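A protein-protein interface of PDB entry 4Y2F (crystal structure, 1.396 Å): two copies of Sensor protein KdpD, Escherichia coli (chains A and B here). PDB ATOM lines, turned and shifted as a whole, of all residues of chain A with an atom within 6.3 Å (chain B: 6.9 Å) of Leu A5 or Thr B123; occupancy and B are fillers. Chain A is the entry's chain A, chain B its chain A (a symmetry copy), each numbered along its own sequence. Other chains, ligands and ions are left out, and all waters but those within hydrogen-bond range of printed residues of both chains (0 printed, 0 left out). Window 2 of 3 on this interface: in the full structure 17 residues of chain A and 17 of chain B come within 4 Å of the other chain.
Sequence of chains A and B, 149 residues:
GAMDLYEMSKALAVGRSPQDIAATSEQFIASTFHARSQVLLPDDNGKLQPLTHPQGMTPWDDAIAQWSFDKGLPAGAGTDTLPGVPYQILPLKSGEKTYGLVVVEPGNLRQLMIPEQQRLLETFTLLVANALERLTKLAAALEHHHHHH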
ATOM      1  N   GLY A   1     -12.346 -21.430 -13.595  1.00  0.00           N
ATOM      2  CA  GLY A   1     -12.721 -20.096 -14.043  1.00  0.00           C
ATOM      3  C   GLY A   1     -13.368 -20.054 -15.420  1.00  0.00           C
ATOM      4  O   GLY A   1     -13.291 -21.011 -16.201  1.00  0.00           O
ATOM      5  N   ALA A   2     -13.994 -18.907 -15.711  1.00  0.00           N
ATOM      6  CA  ALA A   2     -14.746 -18.721 -16.948  1.00  0.00           C
ATOM      7  C   ALA A   2     -13.878 -18.926 -18.181  1.00  0.00           C
ATOM      8  O   ALA A   2     -14.342 -19.466 -19.192  1.00  0.00           O
ATOM      9  CB  ALA A   2     -15.348 -17.318 -16.968  1.00  0.00           C
ATOM     10  N   MET A   3     -12.621 -18.496 -18.130  1.00  0.00           N
ATOM     11  CA  MET A   3     -11.795 -18.559 -19.328  1.00  0.00           C
ATOM     12  C   MET A   3     -10.969 -19.832 -19.421  1.00  0.00           C
ATOM     13  O   MET A   3     -10.268 -20.021 -20.422  1.00  0.00           O
ATOM     14  CB  MET A   3     -10.884 -17.330 -19.424  1.00  0.00           C
ATOM     15  CG  MET A   3     -11.542 -16.086 -20.014  1.00  0.00           C
ATOM     16  SD  MET A   3     -10.474 -14.673 -19.697  1.00  0.00           S
ATOM     17  CE  MET A   3     -11.328 -13.374 -20.550  1.00  0.00           C
ATOM     18  N   ASP A   4     -11.070 -20.723 -18.434  1.00  0.00           N
ATOM     19  CA  ASP A   4     -10.139 -21.849 -18.353  1.00  0.00           C
ATOM     20  C   ASP A   4     -10.323 -22.835 -19.502  1.00  0.00           C
ATOM     21  O   ASP A   4      -9.337 -23.377 -20.022  1.00  0.00           O
ATOM     22  CB  ASP A   4     -10.272 -22.568 -17.011  1.00  0.00           C
ATOM     23  CG  ASP A   4      -9.765 -21.735 -15.850  1.00  0.00           C
ATOM     24  OD1 ASP A   4      -9.256 -20.618 -16.085  1.00  0.00           O
ATOM     25  OD2 ASP A   4      -9.866 -22.209 -14.698  1.00  0.00           O
ATOM     26  N   LEU A   5     -11.570 -23.108 -19.893  1.00  0.00           N
ATOM     27  CA  LEU A   5     -11.807 -24.058 -20.971  1.00  0.00           C
ATOM     28  C   LEU A   5     -11.174 -23.567 -22.267  1.00  0.00           C
ATOM     29  O   LEU A   5     -10.520 -24.333 -22.987  1.00  0.00           O
ATOM     30  CB  LEU A   5     -13.310 -24.249 -21.156  1.00  0.00           C
ATOM     31  CG  LEU A   5     -13.674 -25.381 -22.105  1.00  0.00           C
ATOM     32  CD1 LEU A   5     -13.484 -26.711 -21.388  1.00  0.00           C
ATOM     33  CD2 LEU A   5     -15.100 -25.220 -22.587  1.00  0.00           C
ATOM     34  N   TYR A   6     -11.372 -22.284 -22.577  1.00  0.00           N
ATOM     35  CA  TYR A   6     -10.768 -21.681 -23.760  1.00  0.00           C
ATOM     36  C   TYR A   6      -9.245 -21.724 -23.687  1.00  0.00           C
ATOM     37  O   TYR A   6      -8.584 -22.041 -24.684  1.00  0.00           O
ATOM     38  CB  TYR A   6     -11.269 -20.244 -23.899  1.00  0.00           C
ATOM     39  CG  TYR A   6     -10.571 -19.434 -24.964  1.00  0.00           C
ATOM     40  CD1 TYR A   6     -11.019 -19.446 -26.275  1.00  0.00           C
ATOM     41  CD2 TYR A   6      -9.473 -18.644 -24.651  1.00  0.00           C
ATOM     42  CE1 TYR A   6     -10.388 -18.702 -27.253  1.00  0.00           C
ATOM     43  CE2 TYR A   6      -8.834 -17.901 -25.620  1.00  0.00           C
ATOM     44  CZ  TYR A   6      -9.295 -17.931 -26.918  1.00  0.00           C
ATOM     45  OH  TYR A   6      -8.665 -17.187 -27.889  1.00  0.00           O
ATOM     46  N   GLU A   7      -8.669 -21.407 -22.523  1.00  0.00           N
ATOM     47  CA  GLU A   7      -7.210 -21.425 -22.407  1.00  0.00           C
ATOM     48  C   GLU A   7      -6.658 -22.837 -22.548  1.00  0.00           C
ATOM     49  O   GLU A   7      -5.607 -23.040 -23.174  1.00  0.00           O
ATOM     50  CB  GLU A   7      -6.744 -20.782 -21.101  1.00  0.00           C
ATOM     51  CG  GLU A   7      -6.829 -19.256 -21.096  1.00  0.00           C
ATOM     52  CD  GLU A   7      -5.956 -18.597 -22.158  1.00  0.00           C
ATOM     53  OE1 GLU A   7      -4.790 -19.017 -22.331  1.00  0.00           O
ATOM     54  OE2 GLU A   7      -6.445 -17.658 -22.821  1.00  0.00           O
ATOM     55  N   MET A   8      -7.349 -23.827 -21.981  1.00  0.00           N
ATOM     56  CA  MET A   8      -6.913 -25.203 -22.166  1.00  0.00           C
ATOM     57  C   MET A   8      -7.018 -25.614 -23.627  1.00  0.00           C
ATOM     58  O   MET A   8      -6.126 -26.290 -24.145  1.00  0.00           O
ATOM     59  CB  MET A   8      -7.701 -26.161 -21.275  1.00  0.00           C
ATOM     60  CG  MET A   8      -7.165 -27.601 -21.382  1.00  0.00           C
ATOM     61  SD  MET A   8      -8.068 -28.850 -20.452  1.00  0.00           S
ATOM     62  CE  MET A   8      -9.635 -28.863 -21.324  1.00  0.00           C
ATOM     63  N   SER A   9      -8.073 -25.177 -24.321  1.00  0.00           N
ATOM     64  CA  SER A   9      -8.219 -25.531 -25.733  1.00  0.00           C
ATOM     65  C   SER A   9      -7.055 -24.996 -26.562  1.00  0.00           C
ATOM     66  O   SER A   9      -6.574 -25.671 -27.484  1.00  0.00           O
ATOM     67  CB  SER A   9      -9.565 -25.038 -26.283  1.00  0.00           C
ATOM     68  OG  SER A   9      -9.494 -23.687 -26.714  1.00  0.00           O
ATOM     69  N   LYS A  10      -6.576 -23.788 -26.248  1.00  0.00           N
ATOM     70  CA  LYS A  10      -5.407 -23.261 -26.946  1.00  0.00           C
ATOM     71  C   LYS A  10      -4.182 -24.125 -26.693  1.00  0.00           C
ATOM     72  O   LYS A  10      -3.404 -24.398 -27.619  1.00  0.00           O
ATOM     73  CB  LYS A  10      -5.131 -21.823 -26.510  1.00  0.00           C
ATOM     74  CG  LYS A  10      -6.107 -20.800 -27.070  1.00  0.00           C
ATOM     75  CD  LYS A  10      -6.005 -19.466 -26.333  1.00  0.00           C
ATOM     76  CE  LYS A  10      -4.722 -18.711 -26.637  1.00  0.00           C
ATOM     77  NZ  LYS A  10      -4.718 -17.373 -25.970  1.00  0.00           N
ATOM     78  N   PHE A  28      -4.271 -28.121 -16.221  1.00  0.00           N
ATOM     79  CA  PHE A  28      -5.492 -27.328 -16.201  1.00  0.00           C
ATOM     80  C   PHE A  28      -6.546 -27.930 -15.283  1.00  0.00           C
ATOM     81  O   PHE A  28      -7.281 -27.202 -14.606  1.00  0.00           O
ATOM     82  CB  PHE A  28      -6.036 -27.156 -17.623  1.00  0.00           C
ATOM     83  CG  PHE A  28      -5.389 -26.041 -18.389  1.00  0.00           C
ATOM     84  CD1 PHE A  28      -5.945 -24.768 -18.373  1.00  0.00           C
ATOM     85  CD2 PHE A  28      -4.228 -26.251 -19.113  1.00  0.00           C
ATOM     86  CE1 PHE A  28      -5.352 -23.731 -19.069  1.00  0.00           C
ATOM     87  CE2 PHE A  28      -3.627 -25.214 -19.817  1.00  0.00           C
ATOM     88  CZ  PHE A  28      -4.199 -23.949 -19.796  1.00  0.00           C
ATOM     89  N   THR A  32      -8.010 -25.653 -12.343  1.00  0.00           N
ATOM     90  CA  THR A  32      -9.416 -25.271 -12.414  1.00  0.00           C
ATOM     91  C   THR A  32     -10.238 -25.952 -11.327  1.00  0.00           C
ATOM     92  O   THR A  32     -11.174 -25.354 -10.786  1.00  0.00           O
ATOM     93  CB  THR A  32      -9.973 -25.649 -13.787  1.00  0.00           C
ATOM     94  OG1 THR A  32      -9.226 -24.949 -14.794  1.00  0.00           O
ATOM     95  CG2 THR A  32     -11.458 -25.322 -13.907  1.00  0.00           C
ATOM     96  N   LEU A 120     -18.992 -28.783 -15.618  1.00  0.00           N
ATOM     97  CA  LEU A 120     -17.810 -28.153 -16.205  1.00  0.00           C
ATOM     98  C   LEU A 120     -16.723 -29.184 -16.455  1.00  0.00           C
ATOM     99  O   LEU A 120     -16.086 -29.194 -17.523  1.00  0.00           O
ATOM    100  CB  LEU A 120     -17.299 -27.025 -15.306  1.00  0.00           C
ATOM    101  CG  LEU A 120     -16.060 -26.343 -15.881  1.00  0.00           C
ATOM    102  CD1 LEU A 120     -16.387 -25.645 -17.211  1.00  0.00           C
ATOM    103  CD2 LEU A 120     -15.518 -25.341 -14.879  1.00  0.00           C
ATOM    104  N   THR A 123     -17.211 -31.128 -19.598  1.00  0.00           N
ATOM    105  CA  THR A 123     -16.799 -30.407 -20.794  1.00  0.00           C
ATOM    106  C   THR A 123     -15.290 -30.468 -20.958  1.00  0.00           C
ATOM    107  O   THR A 123     -14.788 -30.652 -22.075  1.00  0.00           O
ATOM    108  CB  THR A 123     -17.273 -28.961 -20.719  1.00  0.00           C
ATOM    109  OG1 THR A 123     -18.696 -28.931 -20.522  1.00  0.00           O
ATOM    110  CG2 THR A 123     -16.953 -28.236 -22.012  1.00  0.00           C
ATOM    111  N   PHE A 124     -14.545 -30.351 -19.853  1.00  0.00           N
ATOM    112  CA  PHE A 124     -13.094 -30.498 -19.933  1.00  0.00           C
ATOM    113  C   PHE A 124     -12.707 -31.863 -20.499  1.00  0.00           C
ATOM    114  O   PHE A 124     -11.867 -31.951 -21.407  1.00  0.00           O
ATOM    115  CB  PHE A 124     -12.460 -30.279 -18.554  1.00  0.00           C
ATOM    116  CG  PHE A 124     -12.140 -28.846 -18.250  1.00  0.00           C
ATOM    117  CD1 PHE A 124     -13.151 -27.916 -18.062  1.00  0.00           C
ATOM    118  CD2 PHE A 124     -10.822 -28.425 -18.142  1.00  0.00           C
ATOM    119  CE1 PHE A 124     -12.851 -26.587 -17.786  1.00  0.00           C
ATOM    120  CE2 PHE A 124     -10.516 -27.105 -17.859  1.00  0.00           C
ATOM    121  CZ  PHE A 124     -11.527 -26.183 -17.695  1.00  0.00           C
ATOM    122  N   LEU A 127     -13.084 -32.063 -24.263  1.00  0.00           N
ATOM    123  CA  LEU A 127     -12.027 -31.403 -25.027  1.00  0.00           C
ATOM    124  C   LEU A 127     -10.739 -32.219 -25.001  1.00  0.00           C
ATOM    125  O   LEU A 127     -10.062 -32.357 -26.030  1.00  0.00           O
ATOM    126  CB  LEU A 127     -11.790 -30.002 -24.471  1.00  0.00           C
ATOM    127  CG  LEU A 127     -12.870 -28.955 -24.687  1.00  0.00           C
ATOM    128  CD1 LEU A 127     -12.223 -27.638 -24.393  1.00  0.00           C
ATOM    129  CD2 LEU A 127     -13.378 -28.960 -26.114  1.00  0.00           C
ATOM    130  N   LEU B   5     -24.757 -30.104 -25.473  1.00  0.00           N
ATOM    131  CA  LEU B   5     -23.363 -30.141 -25.893  1.00  0.00           C
ATOM    132  C   LEU B   5     -22.884 -31.580 -26.035  1.00  0.00           C
ATOM    133  O   LEU B   5     -22.221 -31.936 -27.018  1.00  0.00           O
ATOM    134  CB  LEU B   5     -22.507 -29.397 -24.870  1.00  0.00           C
ATOM    135  CG  LEU B   5     -21.067 -29.183 -25.313  1.00  0.00           C
ATOM    136  CD1 LEU B   5     -21.024 -28.052 -26.332  1.00  0.00           C
ATOM    137  CD2 LEU B   5     -20.194 -28.873 -24.116  1.00  0.00           C
ATOM    138  N   MET B   8     -24.547 -33.163 -29.118  1.00  0.00           N
ATOM    139  CA  MET B   8     -23.896 -32.715 -30.340  1.00  0.00           C
ATOM    140  C   MET B   8     -22.535 -33.375 -30.504  1.00  0.00           C
ATOM    141  O   MET B   8     -22.170 -33.772 -31.613  1.00  0.00           O
ATOM    142  CB  MET B   8     -23.768 -31.193 -30.376  1.00  0.00           C
ATOM    143  CG  MET B   8     -23.185 -30.708 -31.717  1.00  0.00           C
ATOM    144  SD  MET B   8     -22.895 -28.937 -31.854  1.00  0.00           S
ATOM    145  CE  MET B   8     -21.580 -28.709 -30.657  1.00  0.00           C
ATOM    146  N   GLN B 117     -25.676 -17.369 -22.350  1.00  0.00           N
ATOM    147  CA  GLN B 117     -25.881 -18.021 -23.644  1.00  0.00           C
ATOM    148  C   GLN B 117     -24.672 -17.858 -24.549  1.00  0.00           C
ATOM    149  O   GLN B 117     -24.273 -18.806 -25.241  1.00  0.00           O
ATOM    150  CB  GLN B 117     -27.127 -17.470 -24.338  1.00  0.00           C
ATOM    151  CG  GLN B 117     -28.406 -17.800 -23.625  1.00  0.00           C
ATOM    152  CD  GLN B 117     -28.616 -19.287 -23.507  1.00  0.00           C
ATOM    153  OE1 GLN B 117     -28.394 -20.032 -24.460  1.00  0.00           O
ATOM    154  NE2 GLN B 117     -29.022 -19.736 -22.327  1.00  0.00           N
ATOM    155  N   GLN B 118     -24.101 -16.657 -24.583  1.00  0.00           N
ATOM    156  CA  GLN B 118     -22.869 -16.442 -25.350  1.00  0.00           C
ATOM    157  C   GLN B 118     -21.754 -17.381 -24.917  1.00  0.00           C
ATOM    158  O   GLN B 118     -21.009 -17.893 -25.760  1.00  0.00           O
ATOM    159  CB  GLN B 118     -22.413 -14.988 -25.206  1.00  0.00           C
ATOM    160  CG  GLN B 118     -23.346 -14.019 -25.949  1.00  0.00           C
ATOM    161  CD  GLN B 118     -23.240 -14.207 -27.439  1.00  0.00           C
ATOM    162  OE1 GLN B 118     -22.179 -13.915 -28.011  1.00  0.00           O
ATOM    163  NE2 GLN B 118     -24.287 -14.704 -28.067  1.00  0.00           N
ATOM    164  N   ARG B 119     -21.605 -17.619 -23.609  1.00  0.00           N
ATOM    165  CA  ARG B 119     -20.551 -18.518 -23.157  1.00  0.00           C
ATOM    166  C   ARG B 119     -20.834 -19.947 -23.602  1.00  0.00           C
ATOM    167  O   ARG B 119     -19.913 -20.662 -24.023  1.00  0.00           O
ATOM    168  CB  ARG B 119     -20.397 -18.424 -21.637  1.00  0.00           C
ATOM    169  CG  ARG B 119     -19.870 -17.061 -21.182  1.00  0.00           C
ATOM    170  CD  ARG B 119     -19.502 -17.015 -19.698  1.00  0.00           C
ATOM    171  NE  ARG B 119     -20.633 -17.244 -18.799  1.00  0.00           N
ATOM    172  CZ  ARG B 119     -21.408 -16.286 -18.292  1.00  0.00           C
ATOM    173  NH1 ARG B 119     -21.215 -15.012 -18.617  1.00  0.00           N
ATOM    174  NH2 ARG B 119     -22.403 -16.604 -17.477  1.00  0.00           N
ATOM    175  N   LEU B 120     -22.105 -20.360 -23.577  1.00  0.00           N
ATOM    176  CA  LEU B 120     -22.462 -21.694 -24.058  1.00  0.00           C
ATOM    177  C   LEU B 120     -22.202 -21.811 -25.551  1.00  0.00           C
ATOM    178  O   LEU B 120     -21.647 -22.818 -26.024  1.00  0.00           O
ATOM    179  CB  LEU B 120     -23.922 -22.012 -23.729  1.00  0.00           C
ATOM    180  CG  LEU B 120     -24.336 -23.397 -24.220  1.00  0.00           C
ATOM    181  CD1 LEU B 120     -23.540 -24.496 -23.497  1.00  0.00           C
ATOM    182  CD2 LEU B 120     -25.825 -23.592 -23.998  1.00  0.00           C
ATOM    183  N   LEU B 121     -22.574 -20.777 -26.314  1.00  0.00           N
ATOM    184  CA  LEU B 121     -22.365 -20.815 -27.753  1.00  0.00           C
ATOM    185  C   LEU B 121     -20.885 -20.893 -28.087  1.00  0.00           C
ATOM    186  O   LEU B 121     -20.501 -21.577 -29.043  1.00  0.00           O
ATOM    187  CB  LEU B 121     -23.012 -19.590 -28.389  1.00  0.00           C
ATOM    188  CG  LEU B 121     -22.894 -19.467 -29.916  1.00  0.00           C
ATOM    189  CD1 LEU B 121     -23.456 -20.677 -30.630  1.00  0.00           C
ATOM    190  CD2 LEU B 121     -23.633 -18.190 -30.358  1.00  0.00           C
ATOM    191  N   GLU B 122     -20.032 -20.232 -27.301  1.00  0.00           N
ATOM    192  CA  GLU B 122     -18.603 -20.349 -27.556  1.00  0.00           C
ATOM    193  C   GLU B 122     -18.124 -21.784 -27.394  1.00  0.00           C
ATOM    194  O   GLU B 122     -17.297 -22.262 -28.185  1.00  0.00           O
ATOM    195  CB  GLU B 122     -17.813 -19.410 -26.661  1.00  0.00           C
ATOM    196  CG  GLU B 122     -16.331 -19.531 -26.943  1.00  0.00           C
ATOM    197  CD  GLU B 122     -15.525 -18.492 -26.244  1.00  0.00           C
ATOM    198  OE1 GLU B 122     -15.453 -17.359 -26.759  1.00  0.00           O
ATOM    199  OE2 GLU B 122     -14.980 -18.806 -25.170  1.00  0.00           O
ATOM    200  N   THR B 123     -18.636 -22.494 -26.391  1.00  0.00           N
ATOM    201  CA  THR B 123     -18.256 -23.889 -26.217  1.00  0.00           C
ATOM    202  C   THR B 123     -18.723 -24.718 -27.403  1.00  0.00           C
ATOM    203  O   THR B 123     -17.988 -25.588 -27.886  1.00  0.00           O
ATOM    204  CB  THR B 123     -18.843 -24.430 -24.920  1.00  0.00           C
ATOM    205  OG1 THR B 123     -18.422 -23.605 -23.821  1.00  0.00           O
ATOM    206  CG2 THR B 123     -18.355 -25.844 -24.672  1.00  0.00           C
ATOM    207  N   PHE B 124     -19.929 -24.441 -27.911  1.00  0.00           N
ATOM    208  CA  PHE B 124     -20.393 -25.136 -29.109  1.00  0.00           C
ATOM    209  C   PHE B 124     -19.437 -24.916 -30.280  1.00  0.00           C
ATOM    210  O   PHE B 124     -19.048 -25.877 -30.961  1.00  0.00           O
ATOM    211  CB  PHE B 124     -21.812 -24.685 -29.470  1.00  0.00           C
ATOM    212  CG  PHE B 124     -22.894 -25.468 -28.789  1.00  0.00           C
ATOM    213  CD1 PHE B 124     -23.087 -25.371 -27.419  1.00  0.00           C
ATOM    214  CD2 PHE B 124     -23.731 -26.300 -29.520  1.00  0.00           C
ATOM    215  CE1 PHE B 124     -24.087 -26.103 -26.790  1.00  0.00           C
ATOM    216  CE2 PHE B 124     -24.734 -27.025 -28.901  1.00  0.00           C
ATOM    217  CZ  PHE B 124     -24.905 -26.939 -27.536  1.00  0.00           C
ATOM    218  N   THR B 125     -19.037 -23.665 -30.538  1.00  0.00           N
ATOM    219  CA  THR B 125     -18.161 -23.418 -31.681  1.00  0.00           C
ATOM    220  C   THR B 125     -16.801 -24.083 -31.508  1.00  0.00           C
ATOM    221  O   THR B 125     -16.172 -24.468 -32.500  1.00  0.00           O
ATOM    222  CB  THR B 125     -17.993 -21.920 -31.957  1.00  0.00           C
ATOM    223  OG1 THR B 125     -17.305 -21.283 -30.872  1.00  0.00           O
ATOM    224  CG2 THR B 125     -19.345 -21.246 -32.184  1.00  0.00           C
ATOM    225  N   LEU B 126     -16.344 -24.250 -30.264  1.00  0.00           N
ATOM    226  CA  LEU B 126     -15.084 -24.945 -30.037  1.00  0.00           C
ATOM    227  C   LEU B 126     -15.199 -26.419 -30.412  1.00  0.00           C
ATOM    228  O   LEU B 126     -14.292 -26.978 -31.041  1.00  0.00           O
ATOM    229  CB  LEU B 126     -14.681 -24.789 -28.576  1.00  0.00           C
ATOM    230  CG  LEU B 126     -13.432 -25.504 -28.091  1.00  0.00           C
ATOM    231  CD1 LEU B 126     -12.233 -25.135 -28.965  1.00  0.00           C
ATOM    232  CD2 LEU B 126     -13.192 -25.094 -26.662  1.00  0.00           C
ATOM    233  N   LEU B 127     -16.317 -27.055 -30.063  1.00  0.00           N
ATOM    234  CA  LEU B 127     -16.503 -28.459 -30.427  1.00  0.00           C
ATOM    235  C   LEU B 127     -16.644 -28.621 -31.937  1.00  0.00           C
ATOM    236  O   LEU B 127     -16.071 -29.550 -32.525  1.00  0.00           O
ATOM    237  CB  LEU B 127     -17.727 -29.019 -29.707  1.00  0.00           C
ATOM    238  CG  LEU B 127     -17.642 -29.216 -28.203  1.00  0.00           C
ATOM    239  CD1 LEU B 127     -18.792 -30.104 -27.846  1.00  0.00           C
ATOM    240  CD2 LEU B 127     -16.345 -29.884 -27.798  1.00  0.00           C
ATOM    241  N   VAL B 128     -17.370 -27.710 -32.596  1.00  0.00           N
ATOM    242  CA  VAL B 128     -17.466 -27.756 -34.049  1.00  0.00           C
ATOM    243  C   VAL B 128     -16.091 -27.589 -34.687  1.00  0.00           C
ATOM    244  O   VAL B 128     -15.726 -28.315 -35.621  1.00  0.00           O
ATOM    245  CB  VAL B 128     -18.467 -26.701 -34.553  1.00  0.00           C
ATOM    246  CG1 VAL B 128     -18.425 -26.637 -36.072  1.00  0.00           C
ATOM    247  CG2 VAL B 128     -19.867 -27.032 -34.044  1.00  0.00           C
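Among the printed residues, merely in contact across the chains: Leu A5 with Thr B123 (3.9 Å), Ser A9 with Leu B126 (3.6 Å), Thr A123 with Leu B5 (3.9 Å), Thr A123 with Thr B123 (3.8 Å), Leu A127 with Leu B126 (3.5 Å) and Leu A127 with Leu B127 (3.5 Å).
Leu A5 touches Thr B123, and with the chains exchanged Thr A123 touches Leu B5.
Thr B123 touches its own counterpart, Thr A123.
Leu B127 touches its own counterpart, Leu A127.
O of Arg B119 sits at hydrogen-bond distance from OG1 of Thr B123 (3.3 Å).
O of Tyr A6 lies within hydrogen-bond range of OG of Ser A9 (2.8 Å).
Of the printed residues of chain B, Thr A123 touches Leu B5 (3.9 Å) and Thr B123 (3.8 Å).
Of the printed residues of chain B, Leu A127 touches Leu B126 (3.5 Å) and Leu B127 (3.5 Å).
Met B8 touches none of the printed residues of chain A.
Printed residues of chain A within 4 Å of Leu B127: Leu A127 (3.5 Å).
The nearest residue of chain A that does not touch Thr B123 is Leu A127 (6.0 Å).
The nearest printed residue of chain A that does not touch Leu B5 is Leu A5 (6.5 Å).
Of the 16 printed residues of chain A, 4 touch a printed residue of chain B.
Hydrophobic or aromatic side chains of chain A within 4 Å of the printed part of chain B: Leu A5 and Leu A127.
Along chain A the printed residues that touch a printed residue of chain B span positions 5 to 127.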
